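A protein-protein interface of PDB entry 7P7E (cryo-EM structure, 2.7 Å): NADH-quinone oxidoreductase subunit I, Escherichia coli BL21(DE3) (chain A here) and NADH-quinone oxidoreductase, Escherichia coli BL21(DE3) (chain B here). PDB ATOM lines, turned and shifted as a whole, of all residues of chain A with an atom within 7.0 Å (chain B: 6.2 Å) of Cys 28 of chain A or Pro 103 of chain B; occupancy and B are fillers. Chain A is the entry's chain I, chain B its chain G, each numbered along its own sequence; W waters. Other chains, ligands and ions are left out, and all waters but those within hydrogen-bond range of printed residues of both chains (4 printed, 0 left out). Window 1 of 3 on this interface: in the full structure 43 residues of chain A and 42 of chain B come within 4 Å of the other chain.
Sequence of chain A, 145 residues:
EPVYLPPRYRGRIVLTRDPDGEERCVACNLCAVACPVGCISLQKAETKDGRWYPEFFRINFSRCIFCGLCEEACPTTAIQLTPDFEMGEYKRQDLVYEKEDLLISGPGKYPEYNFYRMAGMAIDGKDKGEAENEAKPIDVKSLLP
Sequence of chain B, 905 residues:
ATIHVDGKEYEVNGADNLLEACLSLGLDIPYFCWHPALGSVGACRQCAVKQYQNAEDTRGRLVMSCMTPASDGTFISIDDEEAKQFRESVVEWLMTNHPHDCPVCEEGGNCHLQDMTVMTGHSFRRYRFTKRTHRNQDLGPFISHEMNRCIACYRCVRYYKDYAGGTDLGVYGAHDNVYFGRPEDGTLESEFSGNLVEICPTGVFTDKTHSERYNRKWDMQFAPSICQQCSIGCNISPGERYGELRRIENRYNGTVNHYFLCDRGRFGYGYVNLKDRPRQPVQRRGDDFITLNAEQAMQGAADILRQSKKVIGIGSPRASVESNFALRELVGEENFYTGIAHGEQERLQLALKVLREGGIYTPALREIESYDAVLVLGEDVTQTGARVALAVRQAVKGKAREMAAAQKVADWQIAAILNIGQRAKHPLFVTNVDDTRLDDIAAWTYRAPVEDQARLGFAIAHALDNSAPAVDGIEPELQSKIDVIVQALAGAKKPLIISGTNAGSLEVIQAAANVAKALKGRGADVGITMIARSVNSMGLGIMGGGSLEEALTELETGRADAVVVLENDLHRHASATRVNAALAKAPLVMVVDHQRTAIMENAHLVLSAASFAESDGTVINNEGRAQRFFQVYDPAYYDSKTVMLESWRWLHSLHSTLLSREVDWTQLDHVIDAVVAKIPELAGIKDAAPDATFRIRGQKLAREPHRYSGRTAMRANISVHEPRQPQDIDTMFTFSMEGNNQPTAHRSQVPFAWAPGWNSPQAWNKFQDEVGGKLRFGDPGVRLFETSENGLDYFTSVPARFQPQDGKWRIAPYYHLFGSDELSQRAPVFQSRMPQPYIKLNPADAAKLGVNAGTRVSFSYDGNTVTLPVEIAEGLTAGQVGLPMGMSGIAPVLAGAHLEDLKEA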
ATOM      1  N   CYS A  25       5.797  27.868  20.515  1.00  0.00           N
ATOM      2  CA  CYS A  25       6.534  27.369  21.666  1.00  0.00           C
ATOM      3  C   CYS A  25       5.644  27.311  22.897  1.00  0.00           C
ATOM      4  O   CYS A  25       5.009  28.299  23.272  1.00  0.00           O
ATOM      5  CB  CYS A  25       7.758  28.237  21.943  1.00  0.00           C
ATOM      6  SG  CYS A  25       8.674  27.726  23.407  1.00  0.00           S
ATOM      7  N   VAL A  26       5.600  26.137  23.520  1.00  0.00           N
ATOM      8  CA  VAL A  26       4.830  25.918  24.733  1.00  0.00           C
ATOM      9  C   VAL A  26       5.714  25.945  25.970  1.00  0.00           C
ATOM     10  O   VAL A  26       5.254  25.595  27.061  1.00  0.00           O
ATOM     11  CB  VAL A  26       4.045  24.603  24.649  1.00  0.00           C
ATOM     12  CG1 VAL A  26       3.127  24.623  23.449  1.00  0.00           C
ATOM     13  CG2 VAL A  26       4.996  23.422  24.576  1.00  0.00           C
ATOM     14  N   ALA A  27       6.982  26.342  25.817  1.00  0.00           N
ATOM     15  CA  ALA A  27       7.951  26.467  26.908  1.00  0.00           C
ATOM     16  C   ALA A  27       8.123  25.161  27.676  1.00  0.00           C
ATOM     17  O   ALA A  27       8.168  25.141  28.906  1.00  0.00           O
ATOM     18  CB  ALA A  27       7.582  27.610  27.850  1.00  0.00           C
ATOM     19  N   CYS A  28       8.220  24.059  26.939  1.00  0.00           N
ATOM     20  CA  CYS A  28       8.304  22.739  27.541  1.00  0.00           C
ATOM     21  C   CYS A  28       9.716  22.358  27.966  1.00  0.00           C
ATOM     22  O   CYS A  28       9.883  21.313  28.603  1.00  0.00           O
ATOM     23  CB  CYS A  28       7.763  21.704  26.564  1.00  0.00           C
ATOM     24  SG  CYS A  28       8.908  21.220  25.277  1.00  0.00           S
ATOM     25  N   ASN A  29      10.719  23.161  27.603  1.00  0.00           N
ATOM     26  CA  ASN A  29      12.115  23.029  28.026  1.00  0.00           C
ATOM     27  C   ASN A  29      12.782  21.748  27.532  1.00  0.00           C
ATOM     28  O   ASN A  29      13.784  21.317  28.104  1.00  0.00           O
ATOM     29  CB  ASN A  29      12.257  23.131  29.550  1.00  0.00           C
ATOM     30  CG  ASN A  29      12.741  24.486  29.997  1.00  0.00           C
ATOM     31  OD1 ASN A  29      13.914  24.816  29.849  1.00  0.00           O
ATOM     32  ND2 ASN A  29      11.840  25.280  30.552  1.00  0.00           N
ATOM     33  N   LEU A  30      12.268  21.123  26.473  1.00  0.00           N
ATOM     34  CA  LEU A  30      12.949  19.950  25.932  1.00  0.00           C
ATOM     35  C   LEU A  30      14.176  20.335  25.111  1.00  0.00           C
ATOM     36  O   LEU A  30      15.182  19.618  25.123  1.00  0.00           O
ATOM     37  CB  LEU A  30      11.984  19.117  25.090  1.00  0.00           C
ATOM     38  CG  LEU A  30      10.987  18.251  25.863  1.00  0.00           C
ATOM     39  CD1 LEU A  30      10.211  17.364  24.909  1.00  0.00           C
ATOM     40  CD2 LEU A  30      11.684  17.423  26.926  1.00  0.00           C
ATOM     41  N   CYS A  31      14.112  21.460  24.395  1.00  0.00           N
ATOM     42  CA  CYS A  31      15.255  21.901  23.600  1.00  0.00           C
ATOM     43  C   CYS A  31      16.425  22.306  24.483  1.00  0.00           C
ATOM     44  O   CYS A  31      17.585  22.068  24.129  1.00  0.00           O
ATOM     45  CB  CYS A  31      14.857  23.064  22.696  1.00  0.00           C
ATOM     46  SG  CYS A  31      14.212  24.495  23.566  1.00  0.00           S
ATOM     47  N   ALA A  32      16.139  22.938  25.624  1.00  0.00           N
ATOM     48  CA  ALA A  32      17.197  23.386  26.522  1.00  0.00           C
ATOM     49  C   ALA A  32      17.960  22.209  27.115  1.00  0.00           C
ATOM     50  O   ALA A  32      19.191  22.251  27.217  1.00  0.00           O
ATOM     51  CB  ALA A  32      16.608  24.257  27.628  1.00  0.00           C
ATOM     52  N   VAL A  33      17.254  21.149  27.501  1.00  0.00           N
ATOM     53  CA  VAL A  33      17.932  19.993  28.073  1.00  0.00           C
ATOM     54  C   VAL A  33      18.563  19.137  26.978  1.00  0.00           C
ATOM     55  O   VAL A  33      19.589  18.489  27.209  1.00  0.00           O
ATOM     56  CB  VAL A  33      16.955  19.203  28.966  1.00  0.00           C
ATOM     57  CG1 VAL A  33      15.793  18.655  28.169  1.00  0.00           C
ATOM     58  CG2 VAL A  33      17.665  18.105  29.742  1.00  0.00           C
ATOM     59  N   LEU A  42      15.118  29.346  29.061  1.00  0.00           N
ATOM     60  CA  LEU A  42      13.760  29.838  28.900  1.00  0.00           C
ATOM     61  C   LEU A  42      12.979  29.585  30.180  1.00  0.00           C
ATOM     62  O   LEU A  42      13.366  28.765  31.015  1.00  0.00           O
ATOM     63  CB  LEU A  42      13.072  29.174  27.703  1.00  0.00           C
ATOM     64  CG  LEU A  42      12.846  27.669  27.840  1.00  0.00           C
ATOM     65  CD1 LEU A  42      11.370  27.382  27.846  1.00  0.00           C
ATOM     66  CD2 LEU A  42      13.536  26.898  26.732  1.00  0.00           C
ATOM     67  N   LYS A  44       8.789  29.126  31.534  1.00  0.00           N
ATOM     68  CA  LYS A  44       7.385  28.979  31.188  1.00  0.00           C
ATOM     69  C   LYS A  44       6.543  30.052  31.867  1.00  0.00           C
ATOM     70  O   LYS A  44       6.710  30.325  33.059  1.00  0.00           O
ATOM     71  CB  LYS A  44       6.891  27.588  31.580  1.00  0.00           C
ATOM     72  CG  LYS A  44       5.392  27.391  31.461  1.00  0.00           C
ATOM     73  CD  LYS A  44       4.760  27.185  32.822  1.00  0.00           C
ATOM     74  CE  LYS A  44       3.255  27.283  32.750  1.00  0.00           C
ATOM     75  NZ  LYS A  44       2.611  26.650  33.927  1.00  0.00           N
ATOM     76  N   TRP A  52       0.338  27.742  27.599  1.00  0.00           N
ATOM     77  CA  TRP A  52       1.747  27.841  27.950  1.00  0.00           C
ATOM     78  C   TRP A  52       2.514  28.565  26.852  1.00  0.00           C
ATOM     79  O   TRP A  52       2.263  28.362  25.663  1.00  0.00           O
ATOM     80  CB  TRP A  52       2.349  26.452  28.155  1.00  0.00           C
ATOM     81  CG  TRP A  52       1.965  25.742  29.417  1.00  0.00           C
ATOM     82  CD1 TRP A  52       0.794  25.856  30.104  1.00  0.00           C
ATOM     83  CD2 TRP A  52       2.756  24.786  30.129  1.00  0.00           C
ATOM     84  NE1 TRP A  52       0.811  25.037  31.203  1.00  0.00           N
ATOM     85  CE2 TRP A  52       2.004  24.367  31.241  1.00  0.00           C
ATOM     86  CE3 TRP A  52       4.032  24.245  29.936  1.00  0.00           C
ATOM     87  CZ2 TRP A  52       2.485  23.437  32.158  1.00  0.00           C
ATOM     88  CZ3 TRP A  52       4.505  23.323  30.844  1.00  0.00           C
ATOM     89  CH2 TRP A  52       3.734  22.927  31.942  1.00  0.00           C
ATOM     90  N   TYR A  53       3.461  29.404  27.253  1.00  0.00           N
ATOM     91  CA  TYR A  53       4.306  30.128  26.317  1.00  0.00           C
ATOM     92  C   TYR A  53       5.603  30.476  27.032  1.00  0.00           C
ATOM     93  O   TYR A  53       5.672  30.390  28.261  1.00  0.00           O
ATOM     94  CB  TYR A  53       3.597  31.384  25.781  1.00  0.00           C
ATOM     95  CG  TYR A  53       3.500  32.528  26.757  1.00  0.00           C
ATOM     96  CD1 TYR A  53       2.536  32.534  27.754  1.00  0.00           C
ATOM     97  CD2 TYR A  53       4.360  33.611  26.669  1.00  0.00           C
ATOM     98  CE1 TYR A  53       2.445  33.580  28.645  1.00  0.00           C
ATOM     99  CE2 TYR A  53       4.277  34.660  27.556  1.00  0.00           C
ATOM    100  CZ  TYR A  53       3.315  34.641  28.540  1.00  0.00           C
ATOM    101  OH  TYR A  53       3.227  35.687  29.426  1.00  0.00           O
ATOM    102  N   PRO A  54       6.670  30.800  26.296  1.00  0.00           N
ATOM    103  CA  PRO A  54       7.909  31.209  26.976  1.00  0.00           C
ATOM    104  C   PRO A  54       7.827  32.656  27.444  1.00  0.00           C
ATOM    105  O   PRO A  54       7.546  33.560  26.656  1.00  0.00           O
ATOM    106  CB  PRO A  54       8.983  31.024  25.899  1.00  0.00           C
ATOM    107  CG  PRO A  54       8.255  31.131  24.623  1.00  0.00           C
ATOM    108  CD  PRO A  54       6.903  30.541  24.865  1.00  0.00           C
ATOM    109  N   ALA A  73      14.456  17.824  19.047  1.00  0.00           N
ATOM    110  CA  ALA A  73      13.759  17.531  20.290  1.00  0.00           C
ATOM    111  C   ALA A  73      12.464  18.311  20.468  1.00  0.00           C
ATOM    112  O   ALA A  73      11.721  18.015  21.408  1.00  0.00           O
ATOM    113  CB  ALA A  73      14.673  17.808  21.478  1.00  0.00           C
ATOM    114  N   CYS A  74      12.174  19.281  19.612  1.00  0.00           N
ATOM    115  CA  CYS A  74      10.984  20.107  19.796  1.00  0.00           C
ATOM    116  C   CYS A  74       9.725  19.318  19.472  1.00  0.00           C
ATOM    117  O   CYS A  74       9.603  18.795  18.359  1.00  0.00           O
ATOM    118  CB  CYS A  74      11.052  21.358  18.928  1.00  0.00           C
ATOM    119  SG  CYS A  74       9.777  22.612  19.266  1.00  0.00           S
ATOM    120  N   PRO A  75       8.776  19.205  20.397  1.00  0.00           N
ATOM    121  CA  PRO A  75       7.514  18.514  20.112  1.00  0.00           C
ATOM    122  C   PRO A  75       6.434  19.386  19.491  1.00  0.00           C
ATOM    123  O   PRO A  75       5.324  18.895  19.271  1.00  0.00           O
ATOM    124  CB  PRO A  75       7.086  18.045  21.508  1.00  0.00           C
ATOM    125  CG  PRO A  75       7.600  19.108  22.408  1.00  0.00           C
ATOM    126  CD  PRO A  75       8.864  19.637  21.802  1.00  0.00           C
ATOM    127  N   THR A  76       6.711  20.662  19.233  1.00  0.00           N
ATOM    128  CA  THR A  76       5.742  21.562  18.625  1.00  0.00           C
ATOM    129  C   THR A  76       6.223  22.153  17.309  1.00  0.00           C
ATOM    130  O   THR A  76       5.490  22.945  16.706  1.00  0.00           O
ATOM    131  CB  THR A  76       5.388  22.710  19.584  1.00  0.00           C
ATOM    132  OG1 THR A  76       6.467  23.648  19.624  1.00  0.00           O
ATOM    133  CG2 THR A  76       5.125  22.201  20.992  1.00  0.00           C
ATOM    134  N   PHE A 115       0.496  22.131  17.650  1.00  0.00           N
ATOM    135  CA  PHE A 115       0.535  21.234  18.800  1.00  0.00           C
ATOM    136  C   PHE A 115      -0.744  21.333  19.616  1.00  0.00           C
ATOM    137  O   PHE A 115      -1.250  20.321  20.114  1.00  0.00           O
ATOM    138  CB  PHE A 115       1.747  21.541  19.679  1.00  0.00           C
ATOM    139  CG  PHE A 115       1.680  20.912  21.045  1.00  0.00           C
ATOM    140  CD1 PHE A 115       1.935  19.562  21.209  1.00  0.00           C
ATOM    141  CD2 PHE A 115       1.359  21.668  22.162  1.00  0.00           C
ATOM    142  CE1 PHE A 115       1.870  18.978  22.457  1.00  0.00           C
ATOM    143  CE2 PHE A 115       1.289  21.087  23.410  1.00  0.00           C
ATOM    144  CZ  PHE A 115       1.548  19.743  23.558  1.00  0.00           C
ATOM    145  N   ALA A 119      -3.159  18.588  21.843  1.00  0.00           N
ATOM    146  CA  ALA A 119      -3.131  18.470  23.293  1.00  0.00           C
ATOM    147  C   ALA A 119      -4.534  18.539  23.880  1.00  0.00           C
ATOM    148  O   ALA A 119      -5.383  19.307  23.420  1.00  0.00           O
ATOM    149  CB  ALA A 119      -2.259  19.570  23.895  1.00  0.00           C
ATOM    150  N   HIS B 100      -2.520  14.015  24.710  1.00  0.00           N
ATOM    151  CA  HIS B 100      -1.231  14.363  24.105  1.00  0.00           C
ATOM    152  C   HIS B 100      -0.664  15.600  24.806  1.00  0.00           C
ATOM    153  O   HIS B 100      -0.529  16.682  24.234  1.00  0.00           O
ATOM    154  CB  HIS B 100      -1.432  14.599  22.613  1.00  0.00           C
ATOM    155  CG  HIS B 100      -0.169  14.640  21.813  1.00  0.00           C
ATOM    156  ND1 HIS B 100       0.333  13.536  21.160  1.00  0.00           N
ATOM    157  CD2 HIS B 100       0.673  15.660  21.525  1.00  0.00           C
ATOM    158  CE1 HIS B 100       1.440  13.869  20.521  1.00  0.00           C
ATOM    159  NE2 HIS B 100       1.668  15.152  20.727  1.00  0.00           N
ATOM    160  N   ASP B 101      -0.311  15.422  26.080  1.00  0.00           N
ATOM    161  CA  ASP B 101      -0.183  16.554  26.984  1.00  0.00           C
ATOM    162  C   ASP B 101       1.196  16.763  27.591  1.00  0.00           C
ATOM    163  O   ASP B 101       1.381  17.773  28.275  1.00  0.00           O
ATOM    164  CB  ASP B 101      -1.202  16.428  28.124  1.00  0.00           C
ATOM    165  CG  ASP B 101      -2.385  17.350  27.955  1.00  0.00           C
ATOM    166  OD1 ASP B 101      -2.454  18.055  26.930  1.00  0.00           O
ATOM    167  OD2 ASP B 101      -3.247  17.370  28.855  1.00  0.00           O
ATOM    168  N   CYS B 102       2.158  15.865  27.357  1.00  0.00           N
ATOM    169  CA  CYS B 102       3.454  15.920  28.042  1.00  0.00           C
ATOM    170  C   CYS B 102       4.207  17.251  27.955  1.00  0.00           C
ATOM    171  O   CYS B 102       4.777  17.656  28.982  1.00  0.00           O
ATOM    172  CB  CYS B 102       4.371  14.795  27.535  1.00  0.00           C
ATOM    173  SG  CYS B 102       3.875  13.117  27.897  1.00  0.00           S
ATOM    174  N   PRO B 103       4.289  17.958  26.814  1.00  0.00           N
ATOM    175  CA  PRO B 103       4.967  19.267  26.837  1.00  0.00           C
ATOM    176  C   PRO B 103       4.305  20.307  27.727  1.00  0.00           C
ATOM    177  O   PRO B 103       5.006  21.153  28.292  1.00  0.00           O
ATOM    178  CB  PRO B 103       4.944  19.696  25.365  1.00  0.00           C
ATOM    179  CG  PRO B 103       4.827  18.456  24.621  1.00  0.00           C
ATOM    180  CD  PRO B 103       3.941  17.595  25.426  1.00  0.00           C
ATOM    181  N   VAL B 104       2.983  20.273  27.881  1.00  0.00           N
ATOM    182  CA  VAL B 104       2.286  21.283  28.672  1.00  0.00           C
ATOM    183  C   VAL B 104       1.785  20.676  29.973  1.00  0.00           C
ATOM    184  O   VAL B 104       0.788  21.132  30.540  1.00  0.00           O
ATOM    185  CB  VAL B 104       1.128  21.912  27.879  1.00  0.00           C
ATOM    186  CG1 VAL B 104       1.668  22.858  26.838  1.00  0.00           C
ATOM    187  CG2 VAL B 104       0.276  20.837  27.236  1.00  0.00           C
ATOM    188  N   CYS B 105       2.469  19.646  30.453  1.00  0.00           N
ATOM    189  CA  CYS B 105       2.096  18.955  31.677  1.00  0.00           C
ATOM    190  C   CYS B 105       3.180  19.169  32.718  1.00  0.00           C
ATOM    191  O   CYS B 105       4.367  18.975  32.434  1.00  0.00           O
ATOM    192  CB  CYS B 105       1.893  17.468  31.414  1.00  0.00           C
ATOM    193  SG  CYS B 105       1.327  16.472  32.787  1.00  0.00           S
ATOM    194  N   TYR B 214       6.792  27.386  36.879  1.00  0.00           N
ATOM    195  CA  TYR B 214       7.166  26.004  36.616  1.00  0.00           C
ATOM    196  C   TYR B 214       8.537  25.878  35.963  1.00  0.00           C
ATOM    197  O   TYR B 214       8.934  26.700  35.134  1.00  0.00           O
ATOM    198  CB  TYR B 214       6.119  25.334  35.727  1.00  0.00           C
ATOM    199  CG  TYR B 214       6.429  23.887  35.444  1.00  0.00           C
ATOM    200  CD1 TYR B 214       6.286  22.928  36.432  1.00  0.00           C
ATOM    201  CD2 TYR B 214       6.895  23.483  34.201  1.00  0.00           C
ATOM    202  CE1 TYR B 214       6.583  21.612  36.192  1.00  0.00           C
ATOM    203  CE2 TYR B 214       7.194  22.166  33.949  1.00  0.00           C
ATOM    204  CZ  TYR B 214       7.033  21.233  34.949  1.00  0.00           C
ATOM    205  OH  TYR B 214       7.325  19.913  34.712  1.00  0.00           O
ATOM    206  N   ARG B 216      11.255  22.197  34.976  1.00  0.00           N
ATOM    207  CA  ARG B 216      11.331  20.749  35.022  1.00  0.00           C
ATOM    208  C   ARG B 216      12.301  20.286  36.107  1.00  0.00           C
ATOM    209  O   ARG B 216      13.130  21.050  36.604  1.00  0.00           O
ATOM    210  CB  ARG B 216      11.742  20.205  33.661  1.00  0.00           C
ATOM    211  CG  ARG B 216      10.849  20.688  32.533  1.00  0.00           C
ATOM    212  CD  ARG B 216       9.677  19.754  32.333  1.00  0.00           C
ATOM    213  NE  ARG B 216       8.837  20.161  31.214  1.00  0.00           N
ATOM    214  CZ  ARG B 216       7.549  19.876  31.104  1.00  0.00           C
ATOM    215  NH1 ARG B 216       6.912  19.187  32.034  1.00  0.00           N
ATOM    216  NH2 ARG B 216       6.881  20.293  30.035  1.00  0.00           N
ATOM    217  N   TRP B 218      14.826  18.152  36.055  1.00  0.00           N
ATOM    218  CA  TRP B 218      16.243  18.137  35.709  1.00  0.00           C
ATOM    219  C   TRP B 218      16.879  19.518  35.789  1.00  0.00           C
ATOM    220  O   TRP B 218      18.098  19.614  35.953  1.00  0.00           O
ATOM    221  CB  TRP B 218      16.445  17.551  34.312  1.00  0.00           C
ATOM    222  CG  TRP B 218      15.695  18.253  33.217  1.00  0.00           C
ATOM    223  CD1 TRP B 218      16.015  19.444  32.634  1.00  0.00           C
ATOM    224  CD2 TRP B 218      14.511  17.794  32.559  1.00  0.00           C
ATOM    225  NE1 TRP B 218      15.099  19.759  31.669  1.00  0.00           N
ATOM    226  CE2 TRP B 218      14.168  18.758  31.596  1.00  0.00           C
ATOM    227  CE3 TRP B 218      13.706  16.658  32.692  1.00  0.00           C
ATOM    228  CZ2 TRP B 218      13.059  18.623  30.768  1.00  0.00           C
ATOM    229  CZ3 TRP B 218      12.603  16.533  31.876  1.00  0.00           C
ATOM    230  CH2 TRP B 218      12.285  17.513  30.930  1.00  0.00           C
HETATM  231  O   HOH W   1      12.744  23.839  33.106  1.00  0.00           O
HETATM  232  O   HOH W   2       3.509  16.763  19.797  1.00  0.00           O
HETATM  233  O   HOH W   3      10.119  26.937  32.991  1.00  0.00           O
HETATM  234  O   HOH W   4      15.413  22.183  30.334  1.00  0.00           O
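Pro 103 of chain B touches Val 26 of chain A.
Val 26 of chain A touches Val 104 of chain B (CB to CG1, 3.7 Å).
Cys 28 of chain A touches Pro 103 of chain B.
CZ2 of Trp 218 of chain B touches O of Asn 29 of chain A, 3.9 Å away.
Lys 44 of chain A touches Tyr 214 of chain B.
Trp 52 of chain A touches Pro 103 of chain B (CZ3 to O, 3.4 Å).
CZ2 of Trp 52 of chain A touches O of Val 104 of chain B, 3.3 Å away.
N of Cys 105 of chain B touches CH2 of Trp 52 of chain A, 3.8 Å away.
NH2 of Arg 216 of chain B touches CZ3 of Trp 52 of chain A (3.9 Å).
CG of Pro 103 of chain B touches CG of Pro 75 of chain A, 3.6 Å away.
Hydrophobic or aromatic side chains of chain A that line the printed part of chain B: Val 26, Val 33, Trp 52, Pro 75, Phe 115 and Ala 119.
Along chain A the printed residues that touch a printed residue of chain B span positions 26 to 119.
Of the 9 printed residues of chain B, 8 touch a printed residue of chain A.
The guanidinium group of Arg 216 of chain B lies within hydrogen-bond range of the backbone carbonyl oxygen of Cys 28 of chain A (3.0 Å).
The backbone carbonyl oxygen (O) of Cys 105 of chain B is in hydrogen-bond range of the guanidinium group (NH1) of Arg 216 of chain B, at 2.6 Å.
O of Pro 103 of chain B is in hydrogen-bond range of NH2 of Arg 216 of chain B, 2.7 Å away.
The backbone NH (N) of Leu 30 of chain A lies close to the side-chain sulfur (SG) of Cys 28 of chain A, at 3.6 Å.
The side-chain hydroxyl (OH) of Tyr 214 of chain B is in hydrogen-bond range of the guanidinium group (NH1) of Arg 216 of chain B, at 2.8 Å.
Water W3 lies within hydrogen-bond range of the backbone carbonyl oxygen (O) of Tyr 214 of chain B (2.5 Å), the backbone NH (N) of Lys 44 of chain A (2.9 Å) and the side-chain amide nitrogen (ND2) of Asn 29 of chain A (3.4 Å).
Water W2 lies within hydrogen-bond range of NE2 of His 100 of chain B and O of Pro 75 of chain A.
Water W4 bridges NE1 of Trp 218 of chain B (2.8 Å) and O of Asn 29 of chain A (2.9 Å).
Water W1 bridges the backbone NH (N) of Arg 216 of chain B (2.9 Å) and the side-chain amide nitrogen (ND2) of Asn 29 of chain A (3.1 Å).
Pro 103 of chain B touches just these residues of chain A: Val 26 (3.8 Å), Cys 28 (3.3 Å), Trp 52 (3.4 Å), Pro 75 (3.6 Å) and Phe 115 (3.7 Å).
Printed residues of chain A within 4 Å of His 100 of chain B: Phe 115 (3.6 Å) and Ala 119 (3.3 Å).
Of the printed residues of chain A, Trp 218 of chain B touches Asn 29 (3.9 Å) and Val 33 (3.3 Å).
Printed residues of chain B within 4 Å of Val 33 of chain A: Trp 218 (3.3 Å).
Of the printed residues of chain B, Lys 44 of chain A touches Tyr 214 (3.7 Å).
Leu 42 of chain A touches none of the printed residues of chain B.
Thr 76 of chain A touches none of the printed residues of chain B.
The nearest residue of chain B that does not touch Cys 28 of chain A is Trp 218 of chain B (4.7 Å).
The nearest residue of chain A that does not touch Pro 103 of chain B is Thr 76 of chain A (5.0 Å).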
